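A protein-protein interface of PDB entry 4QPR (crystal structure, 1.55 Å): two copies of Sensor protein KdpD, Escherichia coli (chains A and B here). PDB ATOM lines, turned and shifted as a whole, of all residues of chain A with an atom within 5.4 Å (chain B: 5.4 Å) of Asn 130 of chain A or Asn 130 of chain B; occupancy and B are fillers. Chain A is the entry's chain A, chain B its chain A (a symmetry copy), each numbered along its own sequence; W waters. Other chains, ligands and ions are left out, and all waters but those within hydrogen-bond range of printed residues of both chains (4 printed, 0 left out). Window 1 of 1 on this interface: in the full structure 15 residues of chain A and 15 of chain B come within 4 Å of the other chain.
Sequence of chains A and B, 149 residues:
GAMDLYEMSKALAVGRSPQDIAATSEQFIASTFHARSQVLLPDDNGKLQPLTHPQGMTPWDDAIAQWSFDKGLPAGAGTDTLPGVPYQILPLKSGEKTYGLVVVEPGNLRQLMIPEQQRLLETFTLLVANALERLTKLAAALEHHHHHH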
ATOM      1  N   SER A  94     -17.165  10.573   9.513  1.00  0.00           N
ATOM      2  CA  SER A  94     -17.482  11.434  10.634  1.00  0.00           C
ATOM      3  C   SER A  94     -18.961  11.734  10.536  1.00  0.00           C
ATOM      4  O   SER A  94     -19.411  12.371   9.576  1.00  0.00           O
ATOM      5  CB  SER A  94     -16.675  12.717  10.558  1.00  0.00           C
ATOM      6  OG  SER A  94     -17.068  13.574  11.601  1.00  0.00           O
ATOM      7  N   THR A 125     -10.150   4.983  12.813  1.00  0.00           N
ATOM      8  CA  THR A 125     -10.765   5.521  11.596  1.00  0.00           C
ATOM      9  C   THR A 125     -11.569   6.788  11.883  1.00  0.00           C
ATOM     10  O   THR A 125     -11.613   7.679  11.030  1.00  0.00           O
ATOM     11  CB  THR A 125     -11.624   4.494  10.834  1.00  0.00           C
ATOM     12  OG1 THR A 125     -12.790   4.145  11.591  1.00  0.00           O
ATOM     13  CG2 THR A 125     -10.814   3.247  10.511  1.00  0.00           C
ATOM     14  N   LEU A 126     -12.156   6.889  13.078  1.00  0.00           N
ATOM     15  CA  LEU A 126     -12.879   8.098  13.487  1.00  0.00           C
ATOM     16  C   LEU A 126     -11.932   9.297  13.568  1.00  0.00           C
ATOM     17  O   LEU A 126     -12.268  10.397  13.113  1.00  0.00           O
ATOM     18  CB  LEU A 126     -13.548   7.899  14.849  1.00  0.00           C
ATOM     19  CG  LEU A 126     -14.779   7.010  14.970  1.00  0.00           C
ATOM     20  CD1 LEU A 126     -15.348   7.101  16.387  1.00  0.00           C
ATOM     21  CD2 LEU A 126     -15.822   7.419  13.949  1.00  0.00           C
ATOM     22  N   LEU A 127     -10.752   9.080  14.140  1.00  0.00           N
ATOM     23  CA  LEU A 127      -9.803  10.185  14.308  1.00  0.00           C
ATOM     24  C   LEU A 127      -9.269  10.613  12.940  1.00  0.00           C
ATOM     25  O   LEU A 127      -9.115  11.814  12.658  1.00  0.00           O
ATOM     26  CB  LEU A 127      -8.662   9.815  15.261  1.00  0.00           C
ATOM     27  CG  LEU A 127      -8.920  10.132  16.731  1.00  0.00           C
ATOM     28  CD1 LEU A 127     -10.105   9.381  17.283  1.00  0.00           C
ATOM     29  CD2 LEU A 127      -7.663   9.843  17.534  1.00  0.00           C
ATOM     30  N   VAL A 128      -8.988   9.633  12.085  1.00  0.00           N
ATOM     31  CA  VAL A 128      -8.564   9.942  10.730  1.00  0.00           C
ATOM     32  C   VAL A 128      -9.649  10.725   9.977  1.00  0.00           C
ATOM     33  O   VAL A 128      -9.368  11.729   9.306  1.00  0.00           O
ATOM     34  CB  VAL A 128      -8.168   8.667   9.961  1.00  0.00           C
ATOM     35  CG1 VAL A 128      -7.842   9.013   8.515  1.00  0.00           C
ATOM     36  CG2 VAL A 128      -6.990   7.980  10.638  1.00  0.00           C
ATOM     37  N   ALA A 129     -10.893  10.270  10.083  1.00  0.00           N
ATOM     38  CA  ALA A 129     -12.000  10.959   9.429  1.00  0.00           C
ATOM     39  C   ALA A 129     -12.120  12.389   9.920  1.00  0.00           C
ATOM     40  O   ALA A 129     -12.366  13.298   9.127  1.00  0.00           O
ATOM     41  CB  ALA A 129     -13.288  10.217   9.686  1.00  0.00           C
ATOM     42  N   ASN A 130     -11.940  12.590  11.224  1.00  0.00           N
ATOM     43  CA  ASN A 130     -12.026  13.950  11.769  1.00  0.00           C
ATOM     44  C   ASN A 130     -10.963  14.866  11.172  1.00  0.00           C
ATOM     45  O   ASN A 130     -11.226  16.044  10.922  1.00  0.00           O
ATOM     46  CB  ASN A 130     -11.875  13.950  13.294  1.00  0.00           C
ATOM     47  CG  ASN A 130     -13.119  13.488  14.015  1.00  0.00           C
ATOM     48  OD1 ASN A 130     -14.188  13.348  13.422  1.00  0.00           O
ATOM     49  ND2 ASN A 130     -12.991  13.271  15.319  1.00  0.00           N
ATOM     50  N   ALA A 131      -9.763  14.335  10.960  1.00  0.00           N
ATOM     51  CA  ALA A 131      -8.685  15.137  10.380  1.00  0.00           C
ATOM     52  C   ALA A 131      -9.007  15.477   8.931  1.00  0.00           C
ATOM     53  O   ALA A 131      -8.838  16.623   8.500  1.00  0.00           O
ATOM     54  CB  ALA A 131      -7.351  14.404  10.480  1.00  0.00           C
ATOM     55  N   LEU A 132      -9.484  14.486   8.181  1.00  0.00           N
ATOM     56  CA  LEU A 132      -9.850  14.725   6.789  1.00  0.00           C
ATOM     57  C   LEU A 132     -10.983  15.734   6.680  1.00  0.00           C
ATOM     58  O   LEU A 132     -10.982  16.586   5.802  1.00  0.00           O
ATOM     59  CB  LEU A 132     -10.268  13.418   6.108  1.00  0.00           C
ATOM     60  CG  LEU A 132      -9.118  12.448   5.863  1.00  0.00           C
ATOM     61  CD1 LEU A 132      -9.713  11.134   5.347  1.00  0.00           C
ATOM     62  CD2 LEU A 132      -8.106  13.025   4.882  1.00  0.00           C
ATOM     63  N   GLU A 133     -11.943  15.638   7.596  1.00  0.00           N
ATOM     64  CA  GLU A 133     -13.081  16.557   7.627  1.00  0.00           C
ATOM     65  C   GLU A 133     -12.603  17.979   7.883  1.00  0.00           C
ATOM     66  O   GLU A 133     -13.023  18.917   7.216  1.00  0.00           O
ATOM     67  CB  GLU A 133     -14.058  16.117   8.722  1.00  0.00           C
ATOM     68  CG  GLU A 133     -15.251  17.043   8.954  1.00  0.00           C
ATOM     69  CD  GLU A 133     -16.091  16.577  10.133  1.00  0.00           C
ATOM     70  OE1 GLU A 133     -15.579  15.774  10.936  1.00  0.00           O
ATOM     71  OE2 GLU A 133     -17.254  17.001  10.246  1.00  0.00           O
ATOM     72  N   ARG A 134     -11.717  18.130   8.865  1.00  0.00           N
ATOM     73  CA  ARG A 134     -11.173  19.448   9.176  1.00  0.00           C
ATOM     74  C   ARG A 134     -10.472  20.058   7.967  1.00  0.00           C
ATOM     75  O   ARG A 134     -10.715  21.209   7.620  1.00  0.00           O
ATOM     76  CB  ARG A 134     -10.206  19.369  10.359  1.00  0.00           C
ATOM     77  CG  ARG A 134      -9.622  20.713  10.756  1.00  0.00           C
ATOM     78  CD  ARG A 134      -8.703  20.574  11.954  1.00  0.00           C
ATOM     79  NE  ARG A 134      -7.503  19.805  11.635  1.00  0.00           N
ATOM     80  CZ  ARG A 134      -7.224  18.601  12.120  1.00  0.00           C
ATOM     81  NH1 ARG A 134      -8.076  17.985  12.948  1.00  0.00           N
ATOM     82  NH2 ARG A 134      -6.090  18.001  11.768  1.00  0.00           N
ATOM     83  N   LEU A 135      -9.612  19.282   7.316  1.00  0.00           N
ATOM     84  CA  LEU A 135      -8.862  19.817   6.180  1.00  0.00           C
ATOM     85  C   LEU A 135      -9.750  20.146   4.982  1.00  0.00           C
ATOM     86  O   LEU A 135      -9.556  21.163   4.310  1.00  0.00           O
ATOM     87  CB  LEU A 135      -7.736  18.871   5.767  1.00  0.00           C
ATOM     88  CG  LEU A 135      -6.536  18.850   6.710  1.00  0.00           C
ATOM     89  CD1 LEU A 135      -5.441  17.973   6.146  1.00  0.00           C
ATOM     90  CD2 LEU A 135      -6.018  20.259   6.949  1.00  0.00           C
ATOM     91  N   SER B  94      -6.155  18.938  21.283  1.00  0.00           N
ATOM     92  CA  SER B  94      -5.851  18.291  20.023  1.00  0.00           C
ATOM     93  C   SER B  94      -4.414  18.635  19.702  1.00  0.00           C
ATOM     94  O   SER B  94      -4.081  19.806  19.487  1.00  0.00           O
ATOM     95  CB  SER B  94      -6.774  18.802  18.932  1.00  0.00           C
ATOM     96  OG  SER B  94      -6.400  18.231  17.703  1.00  0.00           O
ATOM     97  N   THR B 125     -12.429  13.052  25.446  1.00  0.00           N
ATOM     98  CA  THR B 125     -11.938  14.433  25.415  1.00  0.00           C
ATOM     99  C   THR B 125     -11.236  14.753  24.097  1.00  0.00           C
ATOM    100  O   THR B 125     -11.323  15.891  23.629  1.00  0.00           O
ATOM    101  CB  THR B 125     -11.036  14.793  26.611  1.00  0.00           C
ATOM    102  OG1 THR B 125      -9.800  14.068  26.553  1.00  0.00           O
ATOM    103  CG2 THR B 125     -11.747  14.514  27.927  1.00  0.00           C
ATOM    104  N   LEU B 126     -10.592  13.757  23.484  1.00  0.00           N
ATOM    105  CA  LEU B 126      -9.958  13.935  22.172  1.00  0.00           C
ATOM    106  C   LEU B 126     -11.003  14.257  21.102  1.00  0.00           C
ATOM    107  O   LEU B 126     -10.796  15.143  20.265  1.00  0.00           O
ATOM    108  CB  LEU B 126      -9.195  12.674  21.760  1.00  0.00           C
ATOM    109  CG  LEU B 126      -7.883  12.318  22.448  1.00  0.00           C
ATOM    110  CD1 LEU B 126      -7.243  11.115  21.755  1.00  0.00           C
ATOM    111  CD2 LEU B 126      -6.944  13.508  22.430  1.00  0.00           C
ATOM    112  N   LEU B 127     -12.123  13.542  21.136  1.00  0.00           N
ATOM    113  CA  LEU B 127     -13.156  13.746  20.116  1.00  0.00           C
ATOM    114  C   LEU B 127     -13.806  15.117  20.315  1.00  0.00           C
ATOM    115  O   LEU B 127     -14.085  15.842  19.345  1.00  0.00           O
ATOM    116  CB  LEU B 127     -14.202  12.626  20.133  1.00  0.00           C
ATOM    117  CG  LEU B 127     -13.887  11.437  19.230  1.00  0.00           C
ATOM    118  CD1 LEU B 127     -12.609  10.740  19.620  1.00  0.00           C
ATOM    119  CD2 LEU B 127     -15.064  10.476  19.240  1.00  0.00           C
ATOM    120  N   VAL B 128     -14.048  15.477  21.573  1.00  0.00           N
ATOM    121  CA  VAL B 128     -14.577  16.797  21.868  1.00  0.00           C
ATOM    122  C   VAL B 128     -13.613  17.897  21.398  1.00  0.00           C
ATOM    123  O   VAL B 128     -14.023  18.886  20.772  1.00  0.00           O
ATOM    124  CB  VAL B 128     -14.900  16.951  23.367  1.00  0.00           C
ATOM    125  CG1 VAL B 128     -15.341  18.378  23.660  1.00  0.00           C
ATOM    126  CG2 VAL B 128     -15.970  15.952  23.787  1.00  0.00           C
ATOM    127  N   ALA B 129     -12.329  17.730  21.696  1.00  0.00           N
ATOM    128  CA  ALA B 129     -11.330  18.702  21.269  1.00  0.00           C
ATOM    129  C   ALA B 129     -11.311  18.840  19.759  1.00  0.00           C
ATOM    130  O   ALA B 129     -11.195  19.949  19.239  1.00  0.00           O
ATOM    131  CB  ALA B 129      -9.967  18.287  21.765  1.00  0.00           C
ATOM    132  N   ASN B 130     -11.431  17.715  19.055  1.00  0.00           N
ATOM    133  CA  ASN B 130     -11.437  17.773  17.588  1.00  0.00           C
ATOM    134  C   ASN B 130     -12.611  18.588  17.059  1.00  0.00           C
ATOM    135  O   ASN B 130     -12.471  19.314  16.072  1.00  0.00           O
ATOM    136  CB  ASN B 130     -11.497  16.369  16.977  1.00  0.00           C
ATOM    137  CG  ASN B 130     -10.176  15.639  17.030  1.00  0.00           C
ATOM    138  OD1 ASN B 130      -9.136  16.220  17.336  1.00  0.00           O
ATOM    139  ND2 ASN B 130     -10.206  14.352  16.704  1.00  0.00           N
ATOM    140  N   ALA B 131     -13.769  18.460  17.700  1.00  0.00           N
ATOM    141  CA  ALA B 131     -14.947  19.213  17.269  1.00  0.00           C
ATOM    142  C   ALA B 131     -14.742  20.700  17.530  1.00  0.00           C
ATOM    143  O   ALA B 131     -15.040  21.537  16.671  1.00  0.00           O
ATOM    144  CB  ALA B 131     -16.201  18.707  17.975  1.00  0.00           C
ATOM    145  N   LEU B 132     -14.223  21.028  18.711  1.00  0.00           N
ATOM    146  CA  LEU B 132     -13.963  22.426  19.039  1.00  0.00           C
ATOM    147  C   LEU B 132     -12.934  23.033  18.096  1.00  0.00           C
ATOM    148  O   LEU B 132     -13.064  24.175  17.677  1.00  0.00           O
ATOM    149  CB  LEU B 132     -13.468  22.560  20.482  1.00  0.00           C
ATOM    150  CG  LEU B 132     -14.539  22.289  21.534  1.00  0.00           C
ATOM    151  CD1 LEU B 132     -13.859  22.287  22.906  1.00  0.00           C
ATOM    152  CD2 LEU B 132     -15.655  23.324  21.466  1.00  0.00           C
ATOM    153  N   GLU B 133     -11.917  22.247  17.755  1.00  0.00           N
ATOM    154  CA  GLU B 133     -10.866  22.690  16.837  1.00  0.00           C
ATOM    155  C   GLU B 133     -11.455  22.984  15.465  1.00  0.00           C
ATOM    156  O   GLU B 133     -11.162  24.007  14.857  1.00  0.00           O
ATOM    157  CB  GLU B 133      -9.791  21.603  16.735  1.00  0.00           C
ATOM    158  CG  GLU B 133      -8.676  21.872  15.726  1.00  0.00           C
ATOM    159  CD  GLU B 133      -7.729  20.686  15.622  1.00  0.00           C
ATOM    160  OE1 GLU B 133      -8.118  19.586  16.056  1.00  0.00           O
ATOM    161  OE2 GLU B 133      -6.604  20.859  15.121  1.00  0.00           O
ATOM    162  N   ARG B 134     -12.292  22.070  14.980  1.00  0.00           N
ATOM    163  CA  ARG B 134     -12.934  22.265  13.684  1.00  0.00           C
ATOM    164  C   ARG B 134     -13.757  23.549  13.661  1.00  0.00           C
ATOM    165  O   ARG B 134     -13.640  24.350  12.740  1.00  0.00           O
ATOM    166  CB  ARG B 134     -13.819  21.069  13.331  1.00  0.00           C
ATOM    167  CG  ARG B 134     -14.498  21.194  11.978  1.00  0.00           C
ATOM    168  CD  ARG B 134     -15.328  19.962  11.672  1.00  0.00           C
ATOM    169  NE  ARG B 134     -16.470  19.836  12.573  1.00  0.00           N
ATOM    170  CZ  ARG B 134     -16.610  18.885  13.489  1.00  0.00           C
ATOM    171  NH1 ARG B 134     -15.659  17.961  13.663  1.00  0.00           N
ATOM    172  NH2 ARG B 134     -17.704  18.863  14.246  1.00  0.00           N
ATOM    173  N   LEU B 135     -14.581  23.754  14.684  1.00  0.00           N
ATOM    174  CA  LEU B 135     -15.441  24.936  14.703  1.00  0.00           C
ATOM    175  C   LEU B 135     -14.659  26.240  14.840  1.00  0.00           C
ATOM    176  O   LEU B 135     -14.983  27.243  14.197  1.00  0.00           O
ATOM    177  CB  LEU B 135     -16.499  24.831  15.800  1.00  0.00           C
ATOM    178  CG  LEU B 135     -17.635  23.854  15.506  1.00  0.00           C
ATOM    179  CD1 LEU B 135     -18.677  23.917  16.599  1.00  0.00           C
ATOM    180  CD2 LEU B 135     -18.264  24.155  14.155  1.00  0.00           C
HETATM  181  O   HOH W   1      -8.328  13.760  14.350  1.00  0.00           O
HETATM  182  O   HOH W   2     -14.943  15.010  16.928  1.00  0.00           O
HETATM  183  O   HOH W   3     -12.864  17.603  12.548  1.00  0.00           O
HETATM  184  O   HOH W   4     -10.888  18.605  13.892  1.00  0.00           O
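Among the printed residues, merely in contact across the chains: Leu 127 of chain A with Leu 127 of chain B.
The side-chain hydroxyl of Ser 94 of chain A sits at hydrogen-bond distance from the side-chain carboxylate of Glu 133 of chain A (2.7 Å). OG of Ser 94 of chain B lies within hydrogen-bond range of OE1 of Glu 133 of chain B (2.7 Å). The side-chain amide oxygen of Asn 130 of chain A lies within hydrogen-bond range of the side-chain hydroxyl of Ser 94 of chain A (3.4 Å). OG of Ser 94 of chain B is in hydrogen-bond range of OD1 of Asn 130 of chain B (3.4 Å).
Of the printed residues of chain B, Leu 127 of chain A touches Leu 127. Of the printed residues of chain B, Glu 133 of chain A touches Arg 134. Printed residues of chain B within 4 Å of Arg 134 of chain A: Glu 133 (3.5 Å). Leu 135 of chain A touches none of the printed residues of chain B. Of the printed residues of chain A, Asn 130 of chain B touches Asn 130 (3.3 Å). Of the printed residues of chain A, Glu 133 of chain B touches Arg 134. Of the printed residues of chain A, Arg 134 of chain B touches Glu 133 (3.5 Å). The nearest residue of chain A that does not touch Asn 130 of chain B is Leu 127 of chain A (4.4 Å).
Water W1 lies within hydrogen-bond range of the backbone carbonyl oxygen of Leu 127 of chain A (2.7 Å) and the side-chain amide nitrogen of Asn 130 of chain B (3.1 Å). Water W2 lies within hydrogen-bond range of the backbone carbonyl oxygen of Leu 127 of chain B and the side-chain amide nitrogen of Asn 130 of chain A. Water W3 bridges the backbone carbonyl oxygen (O) of Asn 130 of chain A and the guanidinium group (NH1) of Arg 134 of chain B. Water W4 lies within hydrogen-bond range of the backbone carbonyl oxygen of Asn 130 of chain B and the guanidinium group of Arg 134 of chain A.
The side-chain amide nitrogen of Asn 130 of chain A sits close to the side-chain amide nitrogen of Asn 130 of chain B. The side-chain carboxylate (OE1) of Glu 133 of chain A lies within salt-bridge range of the guanidinium group (NH1) of Arg 134 of chain B (3.5 Å). The guanidinium group (NH1) of Arg 134 of chain A lies within salt-bridge range of the side-chain carboxylate (OE1) of Glu 133 of chain B (3.5 Å).
Leu 127 of chain A touches its own counterpart, Leu 127 of chain B. Asn 130 of chain B touches its own counterpart, Asn 130 of chain A. Glu 133 of chain A touches Arg 134 of chain B, and with the chains exchanged Arg 134 of chain A touches Glu 133 of chain B. Of the 4 pairs that touch across the chains among the printed residues, 4 have their exchanged pair printed and touching as well.
Hydrophobic or aromatic side chains of chain A that line the printed part of chain B: Leu 127. Hydrophobic or aromatic side chains of chain B that line the printed part of chain A: Leu 127. Among the printed residues, 4 pairs touch across the chains. Among the printed residues, Asp or Glu carboxylates within 4 Å of a Lys or Arg side-chain nitrogen of the other chain: Glu 133 of chain A with Arg 134 of chain B (3.5 Å) and Arg 134 of chain A with Glu 133 of chain B (3.5 Å).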
